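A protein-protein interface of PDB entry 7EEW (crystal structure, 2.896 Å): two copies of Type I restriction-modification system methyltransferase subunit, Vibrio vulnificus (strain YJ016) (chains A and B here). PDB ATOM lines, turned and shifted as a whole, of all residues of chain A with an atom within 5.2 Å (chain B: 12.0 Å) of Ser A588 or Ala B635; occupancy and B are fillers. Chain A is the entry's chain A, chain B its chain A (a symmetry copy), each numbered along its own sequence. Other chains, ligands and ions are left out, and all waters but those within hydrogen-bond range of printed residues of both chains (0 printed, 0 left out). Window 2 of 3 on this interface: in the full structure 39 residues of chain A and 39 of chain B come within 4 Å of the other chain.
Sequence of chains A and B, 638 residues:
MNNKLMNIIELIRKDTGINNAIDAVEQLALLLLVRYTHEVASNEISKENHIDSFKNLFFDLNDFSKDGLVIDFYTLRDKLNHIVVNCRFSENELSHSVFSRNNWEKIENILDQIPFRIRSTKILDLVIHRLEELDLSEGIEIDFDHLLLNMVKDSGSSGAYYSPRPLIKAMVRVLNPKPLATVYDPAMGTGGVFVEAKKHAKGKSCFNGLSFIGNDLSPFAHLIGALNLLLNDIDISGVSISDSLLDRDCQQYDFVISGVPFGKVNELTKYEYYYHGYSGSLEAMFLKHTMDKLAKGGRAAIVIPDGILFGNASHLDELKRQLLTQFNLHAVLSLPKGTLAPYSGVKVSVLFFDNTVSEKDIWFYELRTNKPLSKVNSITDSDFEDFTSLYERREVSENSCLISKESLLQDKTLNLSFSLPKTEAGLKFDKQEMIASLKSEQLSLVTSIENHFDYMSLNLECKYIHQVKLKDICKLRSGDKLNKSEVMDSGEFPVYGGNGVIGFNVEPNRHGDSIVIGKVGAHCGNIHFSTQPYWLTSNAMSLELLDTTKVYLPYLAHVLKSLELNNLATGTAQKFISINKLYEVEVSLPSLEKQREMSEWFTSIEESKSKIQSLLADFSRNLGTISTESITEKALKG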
ATOM      1  N   TYR A 464      -3.378  16.974 -21.349  1.00  0.00           N
ATOM      2  CA  TYR A 464      -2.860  17.154 -20.000  1.00  0.00           C
ATOM      3  C   TYR A 464      -3.177  15.928 -19.154  1.00  0.00           C
ATOM      4  O   TYR A 464      -4.340  15.528 -19.039  1.00  0.00           O
ATOM      5  CB  TYR A 464      -3.457  18.407 -19.361  1.00  0.00           C
ATOM      6  CG  TYR A 464      -3.337  19.659 -20.203  1.00  0.00           C
ATOM      7  CD1 TYR A 464      -2.205  19.903 -20.971  1.00  0.00           C
ATOM      8  CD2 TYR A 464      -4.362  20.596 -20.233  1.00  0.00           C
ATOM      9  CE1 TYR A 464      -2.098  21.048 -21.743  1.00  0.00           C
ATOM     10  CE2 TYR A 464      -4.264  21.740 -20.999  1.00  0.00           C
ATOM     11  CZ  TYR A 464      -3.132  21.962 -21.753  1.00  0.00           C
ATOM     12  OH  TYR A 464      -3.038  23.103 -22.516  1.00  0.00           O
ATOM     13  N   HIS A 466      -2.218  15.652 -15.767  1.00  0.00           N
ATOM     14  CA  HIS A 466      -2.564  16.156 -14.448  1.00  0.00           C
ATOM     15  C   HIS A 466      -3.193  17.538 -14.566  1.00  0.00           C
ATOM     16  O   HIS A 466      -3.081  18.214 -15.592  1.00  0.00           O
ATOM     17  CB  HIS A 466      -1.333  16.231 -13.534  1.00  0.00           C
ATOM     18  CG  HIS A 466      -0.539  14.962 -13.466  1.00  0.00           C
ATOM     19  ND1 HIS A 466      -1.019  13.752 -13.918  1.00  0.00           N
ATOM     20  CD2 HIS A 466       0.707  14.720 -12.994  1.00  0.00           C
ATOM     21  CE1 HIS A 466      -0.102  12.819 -13.730  1.00  0.00           C
ATOM     22  NE2 HIS A 466       0.955  13.380 -13.171  1.00  0.00           N
ATOM     23  N   GLN A 467      -3.870  17.948 -13.488  1.00  0.00           N
ATOM     24  CA  GLN A 467      -4.425  19.296 -13.346  1.00  0.00           C
ATOM     25  C   GLN A 467      -4.194  19.678 -11.883  1.00  0.00           C
ATOM     26  O   GLN A 467      -5.108  19.671 -11.054  1.00  0.00           O
ATOM     27  CB  GLN A 467      -5.902  19.354 -13.737  1.00  0.00           C
ATOM     28  CG  GLN A 467      -6.421  20.753 -14.047  1.00  0.00           C
ATOM     29  CD  GLN A 467      -6.697  21.576 -12.801  1.00  0.00           C
ATOM     30  OE1 GLN A 467      -7.353  21.111 -11.868  1.00  0.00           O
ATOM     31  NE2 GLN A 467      -6.196  22.805 -12.783  1.00  0.00           N
ATOM     32  N   VAL A 468      -2.943  20.002 -11.563  1.00  0.00           N
ATOM     33  CA  VAL A 468      -2.528  20.214 -10.182  1.00  0.00           C
ATOM     34  C   VAL A 468      -2.610  21.691  -9.829  1.00  0.00           C
ATOM     35  O   VAL A 468      -2.992  22.525 -10.657  1.00  0.00           O
ATOM     36  CB  VAL A 468      -1.104  19.680  -9.947  1.00  0.00           C
ATOM     37  CG1 VAL A 468      -0.987  18.245 -10.434  1.00  0.00           C
ATOM     38  CG2 VAL A 468      -0.081  20.574 -10.639  1.00  0.00           C
ATOM     39  N   TYR A 555       8.870  24.087 -18.949  1.00  0.00           N
ATOM     40  CA  TYR A 555       7.456  24.116 -19.309  1.00  0.00           C
ATOM     41  C   TYR A 555       6.646  24.878 -18.269  1.00  0.00           C
ATOM     42  O   TYR A 555       5.709  25.607 -18.616  1.00  0.00           O
ATOM     43  CB  TYR A 555       6.910  22.696 -19.474  1.00  0.00           C
ATOM     44  CG  TYR A 555       5.483  22.654 -19.987  1.00  0.00           C
ATOM     45  CD1 TYR A 555       5.216  22.617 -21.349  1.00  0.00           C
ATOM     46  CD2 TYR A 555       4.404  22.657 -19.109  1.00  0.00           C
ATOM     47  CE1 TYR A 555       3.916  22.582 -21.824  1.00  0.00           C
ATOM     48  CE2 TYR A 555       3.102  22.624 -19.574  1.00  0.00           C
ATOM     49  CZ  TYR A 555       2.865  22.586 -20.933  1.00  0.00           C
ATOM     50  OH  TYR A 555       1.571  22.551 -21.403  1.00  0.00           O
ATOM     51  N   VAL A 559       4.416  28.334 -18.704  1.00  0.00           N
ATOM     52  CA  VAL A 559       3.001  28.346 -18.342  1.00  0.00           C
ATOM     53  C   VAL A 559       2.741  29.334 -17.211  1.00  0.00           C
ATOM     54  O   VAL A 559       1.633  29.874 -17.094  1.00  0.00           O
ATOM     55  CB  VAL A 559       2.523  26.923 -17.989  1.00  0.00           C
ATOM     56  CG1 VAL A 559       2.920  26.542 -16.573  1.00  0.00           C
ATOM     57  CG2 VAL A 559       1.020  26.806 -18.175  1.00  0.00           C
ATOM     58  N   SER A 562       2.600  32.532 -19.048  1.00  0.00           N
ATOM     59  CA  SER A 562       1.356  32.667 -19.794  1.00  0.00           C
ATOM     60  C   SER A 562       0.197  33.121 -18.919  1.00  0.00           C
ATOM     61  O   SER A 562      -0.773  33.682 -19.438  1.00  0.00           O
ATOM     62  CB  SER A 562       1.004  31.338 -20.464  1.00  0.00           C
ATOM     63  OG  SER A 562       1.965  30.988 -21.444  1.00  0.00           O
ATOM     64  N   GLU A 586      -3.780  27.557 -10.261  1.00  0.00           N
ATOM     65  CA  GLU A 586      -3.940  26.266 -10.914  1.00  0.00           C
ATOM     66  C   GLU A 586      -3.188  26.244 -12.238  1.00  0.00           C
ATOM     67  O   GLU A 586      -3.190  27.227 -12.985  1.00  0.00           O
ATOM     68  CB  GLU A 586      -5.422  25.957 -11.143  1.00  0.00           C
ATOM     69  CG  GLU A 586      -6.182  25.574  -9.882  1.00  0.00           C
ATOM     70  CD  GLU A 586      -7.646  25.284 -10.149  1.00  0.00           C
ATOM     71  OE1 GLU A 586      -8.460  25.419  -9.212  1.00  0.00           O
ATOM     72  OE2 GLU A 586      -7.980  24.924 -11.297  1.00  0.00           O
ATOM     73  N   VAL A 587      -2.544  25.113 -12.520  1.00  0.00           N
ATOM     74  CA  VAL A 587      -1.756  24.929 -13.734  1.00  0.00           C
ATOM     75  C   VAL A 587      -1.971  23.510 -14.242  1.00  0.00           C
ATOM     76  O   VAL A 587      -1.807  22.544 -13.489  1.00  0.00           O
ATOM     77  CB  VAL A 587      -0.257  25.198 -13.489  1.00  0.00           C
ATOM     78  CG1 VAL A 587       0.169  24.650 -12.132  1.00  0.00           C
ATOM     79  CG2 VAL A 587       0.579  24.584 -14.599  1.00  0.00           C
ATOM     80  N   SER A 588      -2.344  23.384 -15.514  1.00  0.00           N
ATOM     81  CA  SER A 588      -2.535  22.092 -16.158  1.00  0.00           C
ATOM     82  C   SER A 588      -1.300  21.763 -16.985  1.00  0.00           C
ATOM     83  O   SER A 588      -0.856  22.582 -17.795  1.00  0.00           O
ATOM     84  CB  SER A 588      -3.779  22.103 -17.047  1.00  0.00           C
ATOM     85  OG  SER A 588      -4.915  22.546 -16.327  1.00  0.00           O
ATOM     86  N   LEU A 589      -0.751  20.569 -16.783  1.00  0.00           N
ATOM     87  CA  LEU A 589       0.470  20.181 -17.467  1.00  0.00           C
ATOM     88  C   LEU A 589       0.339  18.776 -18.034  1.00  0.00           C
ATOM     89  O   LEU A 589      -0.400  17.947 -17.493  1.00  0.00           O
ATOM     90  CB  LEU A 589       1.695  20.258 -16.535  1.00  0.00           C
ATOM     91  CG  LEU A 589       1.706  19.863 -15.047  1.00  0.00           C
ATOM     92  CD1 LEU A 589       0.951  20.862 -14.167  1.00  0.00           C
ATOM     93  CD2 LEU A 589       1.208  18.444 -14.808  1.00  0.00           C
ATOM     94  N   PRO A 590       1.030  18.487 -19.139  1.00  0.00           N
ATOM     95  CA  PRO A 590       0.958  17.141 -19.721  1.00  0.00           C
ATOM     96  C   PRO A 590       2.074  16.229 -19.239  1.00  0.00           C
ATOM     97  O   PRO A 590       2.580  16.377 -18.121  1.00  0.00           O
ATOM     98  CB  PRO A 590       1.075  17.417 -21.222  1.00  0.00           C
ATOM     99  CG  PRO A 590       1.977  18.609 -21.285  1.00  0.00           C
ATOM    100  CD  PRO A 590       1.690  19.440 -20.048  1.00  0.00           C
ATOM    101  N   PHE A 602       7.876  26.202 -27.435  1.00  0.00           N
ATOM    102  CA  PHE A 602       7.566  27.479 -26.799  1.00  0.00           C
ATOM    103  C   PHE A 602       8.785  28.392 -26.750  1.00  0.00           C
ATOM    104  O   PHE A 602       8.667  29.605 -26.958  1.00  0.00           O
ATOM    105  CB  PHE A 602       7.026  27.249 -25.387  1.00  0.00           C
ATOM    106  CG  PHE A 602       5.583  26.840 -25.343  1.00  0.00           C
ATOM    107  CD1 PHE A 602       4.713  27.199 -26.358  1.00  0.00           C
ATOM    108  CD2 PHE A 602       5.094  26.099 -24.279  1.00  0.00           C
ATOM    109  CE1 PHE A 602       3.382  26.823 -26.315  1.00  0.00           C
ATOM    110  CE2 PHE A 602       3.768  25.722 -24.231  1.00  0.00           C
ATOM    111  CZ  PHE A 602       2.910  26.083 -25.248  1.00  0.00           C
ATOM    112  N   ASP B 430      -8.149  33.654 -29.815  1.00  0.00           N
ATOM    113  CA  ASP B 430      -6.984  33.549 -30.686  1.00  0.00           C
ATOM    114  C   ASP B 430      -7.200  32.359 -31.604  1.00  0.00           C
ATOM    115  O   ASP B 430      -7.523  31.260 -31.170  1.00  0.00           O
ATOM    116  CB  ASP B 430      -5.687  33.420 -29.865  1.00  0.00           C
ATOM    117  CG  ASP B 430      -4.432  33.557 -30.693  1.00  0.00           C
ATOM    118  OD1 ASP B 430      -4.255  32.776 -31.613  1.00  0.00           O
ATOM    119  OD2 ASP B 430      -3.597  34.409 -30.397  1.00  0.00           O
ATOM    120  N   GLN B 432      -6.007  30.834 -35.882  1.00  0.00           N
ATOM    121  CA  GLN B 432      -5.030  30.938 -36.956  1.00  0.00           C
ATOM    122  C   GLN B 432      -5.435  31.946 -38.022  1.00  0.00           C
ATOM    123  O   GLN B 432      -4.748  32.055 -39.042  1.00  0.00           O
ATOM    124  CB  GLN B 432      -4.797  29.566 -37.592  1.00  0.00           C
ATOM    125  CG  GLN B 432      -4.036  28.612 -36.690  1.00  0.00           C
ATOM    126  CD  GLN B 432      -2.714  29.191 -36.225  1.00  0.00           C
ATOM    127  OE1 GLN B 432      -1.848  29.519 -37.035  1.00  0.00           O
ATOM    128  NE2 GLN B 432      -2.556  29.331 -34.913  1.00  0.00           N
ATOM    129  N   ILE B 626       0.621  38.156 -31.035  1.00  0.00           N
ATOM    130  CA  ILE B 626       0.262  36.939 -31.754  1.00  0.00           C
ATOM    131  C   ILE B 626       1.131  35.774 -31.295  1.00  0.00           C
ATOM    132  O   ILE B 626       0.654  34.642 -31.152  1.00  0.00           O
ATOM    133  CB  ILE B 626       0.362  37.165 -33.275  1.00  0.00           C
ATOM    134  CG1 ILE B 626      -1.016  37.476 -33.867  1.00  0.00           C
ATOM    135  CG2 ILE B 626       0.982  35.961 -33.977  1.00  0.00           C
ATOM    136  CD1 ILE B 626      -1.656  38.735 -33.329  1.00  0.00           C
ATOM    137  N   SER B 627       2.414  36.036 -31.036  1.00  0.00           N
ATOM    138  CA  SER B 627       3.316  34.966 -30.626  1.00  0.00           C
ATOM    139  C   SER B 627       3.061  34.542 -29.184  1.00  0.00           C
ATOM    140  O   SER B 627       3.173  33.356 -28.852  1.00  0.00           O
ATOM    141  CB  SER B 627       4.767  35.405 -30.818  1.00  0.00           C
ATOM    142  OG  SER B 627       4.941  36.761 -30.442  1.00  0.00           O
ATOM    143  N   THR B 628       2.718  35.493 -28.311  1.00  0.00           N
ATOM    144  CA  THR B 628       2.462  35.150 -26.915  1.00  0.00           C
ATOM    145  C   THR B 628       1.141  34.404 -26.763  1.00  0.00           C
ATOM    146  O   THR B 628       1.094  33.329 -26.156  1.00  0.00           O
ATOM    147  CB  THR B 628       2.466  36.407 -26.044  1.00  0.00           C
ATOM    148  OG1 THR B 628       2.002  37.526 -26.808  1.00  0.00           O
ATOM    149  CG2 THR B 628       3.863  36.691 -25.515  1.00  0.00           C
ATOM    150  N   GLU B 629       0.056  34.961 -27.308  1.00  0.00           N
ATOM    151  CA  GLU B 629      -1.252  34.334 -27.137  1.00  0.00           C
ATOM    152  C   GLU B 629      -1.319  32.970 -27.812  1.00  0.00           C
ATOM    153  O   GLU B 629      -2.103  32.111 -27.394  1.00  0.00           O
ATOM    154  CB  GLU B 629      -2.349  35.253 -27.672  1.00  0.00           C
ATOM    155  CG  GLU B 629      -2.525  36.528 -26.866  1.00  0.00           C
ATOM    156  CD  GLU B 629      -3.719  37.344 -27.317  1.00  0.00           C
ATOM    157  OE1 GLU B 629      -4.539  36.817 -28.098  1.00  0.00           O
ATOM    158  OE2 GLU B 629      -3.835  38.512 -26.891  1.00  0.00           O
ATOM    159  N   SER B 630      -0.511  32.751 -28.853  1.00  0.00           N
ATOM    160  CA  SER B 630      -0.415  31.415 -29.431  1.00  0.00           C
ATOM    161  C   SER B 630       0.301  30.457 -28.490  1.00  0.00           C
ATOM    162  O   SER B 630      -0.016  29.263 -28.462  1.00  0.00           O
ATOM    163  CB  SER B 630       0.304  31.473 -30.780  1.00  0.00           C
ATOM    164  OG  SER B 630       1.660  31.848 -30.615  1.00  0.00           O
ATOM    165  N   ILE B 631       1.264  30.960 -27.714  1.00  0.00           N
ATOM    166  CA  ILE B 631       1.921  30.131 -26.708  1.00  0.00           C
ATOM    167  C   ILE B 631       0.948  29.786 -25.590  1.00  0.00           C
ATOM    168  O   ILE B 631       0.856  28.630 -25.160  1.00  0.00           O
ATOM    169  CB  ILE B 631       3.178  30.836 -26.165  1.00  0.00           C
ATOM    170  CG1 ILE B 631       4.326  30.748 -27.172  1.00  0.00           C
ATOM    171  CG2 ILE B 631       3.591  30.247 -24.820  1.00  0.00           C
ATOM    172  CD1 ILE B 631       5.618  31.349 -26.662  1.00  0.00           C
ATOM    173  N   THR B 632       0.203  30.783 -25.104  1.00  0.00           N
ATOM    174  CA  THR B 632      -0.786  30.536 -24.061  1.00  0.00           C
ATOM    175  C   THR B 632      -1.912  29.632 -24.544  1.00  0.00           C
ATOM    176  O   THR B 632      -2.601  29.023 -23.719  1.00  0.00           O
ATOM    177  CB  THR B 632      -1.374  31.856 -23.559  1.00  0.00           C
ATOM    178  OG1 THR B 632      -2.301  32.367 -24.526  1.00  0.00           O
ATOM    179  CG2 THR B 632      -0.275  32.880 -23.338  1.00  0.00           C
ATOM    180  N   GLU B 633      -2.113  29.537 -25.860  1.00  0.00           N
ATOM    181  CA  GLU B 633      -3.168  28.687 -26.396  1.00  0.00           C
ATOM    182  C   GLU B 633      -2.929  27.221 -26.056  1.00  0.00           C
ATOM    183  O   GLU B 633      -3.863  26.499 -25.693  1.00  0.00           O
ATOM    184  CB  GLU B 633      -3.260  28.877 -27.910  1.00  0.00           C
ATOM    185  CG  GLU B 633      -4.293  28.002 -28.588  1.00  0.00           C
ATOM    186  CD  GLU B 633      -4.040  27.876 -30.076  1.00  0.00           C
ATOM    187  OE1 GLU B 633      -2.860  27.755 -30.466  1.00  0.00           O
ATOM    188  OE2 GLU B 633      -5.017  27.905 -30.852  1.00  0.00           O
ATOM    189  N   LYS B 634      -1.682  26.765 -26.166  1.00  0.00           N
ATOM    190  CA  LYS B 634      -1.334  25.371 -25.937  1.00  0.00           C
ATOM    191  C   LYS B 634      -0.852  25.093 -24.520  1.00  0.00           C
ATOM    192  O   LYS B 634      -0.658  23.925 -24.166  1.00  0.00           O
ATOM    193  CB  LYS B 634      -0.258  24.928 -26.935  1.00  0.00           C
ATOM    194  CG  LYS B 634      -0.745  24.820 -28.370  1.00  0.00           C
ATOM    195  CD  LYS B 634      -1.702  23.650 -28.539  1.00  0.00           C
ATOM    196  CE  LYS B 634      -2.083  23.461 -29.999  1.00  0.00           C
ATOM    197  NZ  LYS B 634      -2.879  22.222 -30.222  1.00  0.00           N
ATOM    198  N   ALA B 635      -0.656  26.128 -23.703  1.00  0.00           N
ATOM    199  CA  ALA B 635      -0.232  25.943 -22.323  1.00  0.00           C
ATOM    200  C   ALA B 635      -1.376  26.040 -21.325  1.00  0.00           C
ATOM    201  O   ALA B 635      -1.230  25.567 -20.193  1.00  0.00           O
ATOM    202  CB  ALA B 635       0.842  26.973 -21.952  1.00  0.00           C
ATOM    203  N   LEU B 636      -2.502  26.636 -21.712  1.00  0.00           N
ATOM    204  CA  LEU B 636      -3.647  26.806 -20.830  1.00  0.00           C
ATOM    205  C   LEU B 636      -4.893  26.266 -21.512  1.00  0.00           C
ATOM    206  O   LEU B 636      -5.158  26.593 -22.674  1.00  0.00           O
ATOM    207  CB  LEU B 636      -3.850  28.281 -20.461  1.00  0.00           C
ATOM    208  CG  LEU B 636      -2.661  29.027 -19.854  1.00  0.00           C
ATOM    209  CD1 LEU B 636      -3.010  30.491 -19.635  1.00  0.00           C
ATOM    210  CD2 LEU B 636      -2.225  28.382 -18.551  1.00  0.00           C
ATOM    211  N   LYS B 637      -5.652  25.440 -20.791  1.00  0.00           N
ATOM    212  CA  LYS B 637      -6.947  24.982 -21.276  1.00  0.00           C
ATOM    213  C   LYS B 637      -8.076  25.934 -20.906  1.00  0.00           C
ATOM    214  O   LYS B 637      -9.131  25.908 -21.553  1.00  0.00           O
ATOM    215  CB  LYS B 637      -7.249  23.579 -20.731  1.00  0.00           C
ATOM    216  CG  LYS B 637      -8.460  22.901 -21.362  1.00  0.00           C
ATOM    217  CD  LYS B 637      -9.641  22.874 -20.404  1.00  0.00           C
ATOM    218  CE  LYS B 637     -10.965  22.970 -21.146  1.00  0.00           C
ATOM    219  NZ  LYS B 637     -11.148  24.303 -21.786  1.00  0.00           N
ATOM    220  N   GLY B 638      -7.875  26.780 -19.901  1.00  0.00           N
ATOM    221  CA  GLY B 638      -8.890  27.725 -19.477  1.00  0.00           C
ATOM    222  C   GLY B 638      -9.062  27.756 -17.972  1.00  0.00           C
ATOM    223  O   GLY B 638      -8.464  26.953 -17.256  1.00  0.00           O
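The backbone carbonyl oxygen of Lys B634 is in hydrogen-bond range of the side-chain hydroxyl of Tyr A464, 3.0 Å away.
The side-chain hydroxyl (OG1) of Thr B632 sits at hydrogen-bond distance from the backbone carbonyl oxygen (O) of Glu B629 (2.9 Å).
Among the printed residues, pairs that only touch across the chains: Tyr A464 with Ala B635, Tyr A464 with Leu B636, Tyr A464 with Lys B637, Tyr A555 with Lys B634, Tyr A555 with Ala B635, Val A559 with Ala B635, Val A559 with Leu B636, Ser A562 with Ile B631, Ser A562 with Thr B632, Ser A562 with Leu B636, Ser A588 with Ala B635, Phe A602 with Ile B631, Phe A602 with Lys B634 and Phe A602 with Ala B635.
Ser A588 touches just one residue of chain B: Ala B635. Ala B635 touches just these residues of chain A: Tyr A464 (3.6 Å), Tyr A555 (3.95 Å), Val A559 (3.3 Å), Ser A588 (3.8 Å) and Phe A602 (3.9 Å). Tyr A464 touches just these residues of chain B: Lys B634, Ala B635, Leu B636 and Lys B637. No residue of chain B comes within 4 Å of Val A468. Ser A562 touches just these residues of chain B: Ile B631 (3.8 Å), Thr B632 (3.5 Å) and Leu B636 (3.9 Å). No residue of chain B comes within 4 Å of Val A587. No residue of chain B comes within 4 Å of Leu A589. No residue of chain B comes within 4 Å of Pro A590. Printed residues of chain A within 4 Å of Thr B632: Ser A562 (3.5 Å). Printed residues of chain B within 4 Å of Tyr A555: Lys B634 and Ala B635. Of the printed residues of chain A, Leu B636 touches Tyr A464, Val A559 and Ser A562. Of the printed residues of chain A, Lys B634 touches Tyr A464 (3.0 Å), Tyr A555 (3.8 Å) and Phe A602 (3.8 Å). Of the printed residues of chain A, Ile B631 touches Ser A562 (3.8 Å) and Phe A602 (3.3 Å). Thr B628 touches none of the printed residues of chain A.
Of the 13 printed residues of chain A, 6 touch a printed residue of chain B. Printed residues of chain A that touch a printed residue of chain B: Tyr A464, Tyr A555, Val A559, Ser A562, Ser A588 and Phe A602. Hydrophobic or aromatic side chains of chain A that line the printed part of chain B: Tyr A464, Tyr A555, Val A559 and Phe A602. Printed residues of chain B that touch a printed residue of chain A: Ile B631, Thr B632, Lys B634, Ala B635, Leu B636 and Lys B637. Hydrophobic or aromatic side chains of chain B within 4 Å of the printed part of chain A: Ile B631, Ala B635 and Leu B636. Among the printed residues, 15 pairs touch across the chains. Among the printed residues, no Asp or Glu carboxylate lies within 4 Å of a Lys or Arg side-chain nitrogen of the other chain.
No position is printed for both chains. Of the 15 pairs that touch across the chains among the printed residues, none has its exchanged pair printed and touching as well.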
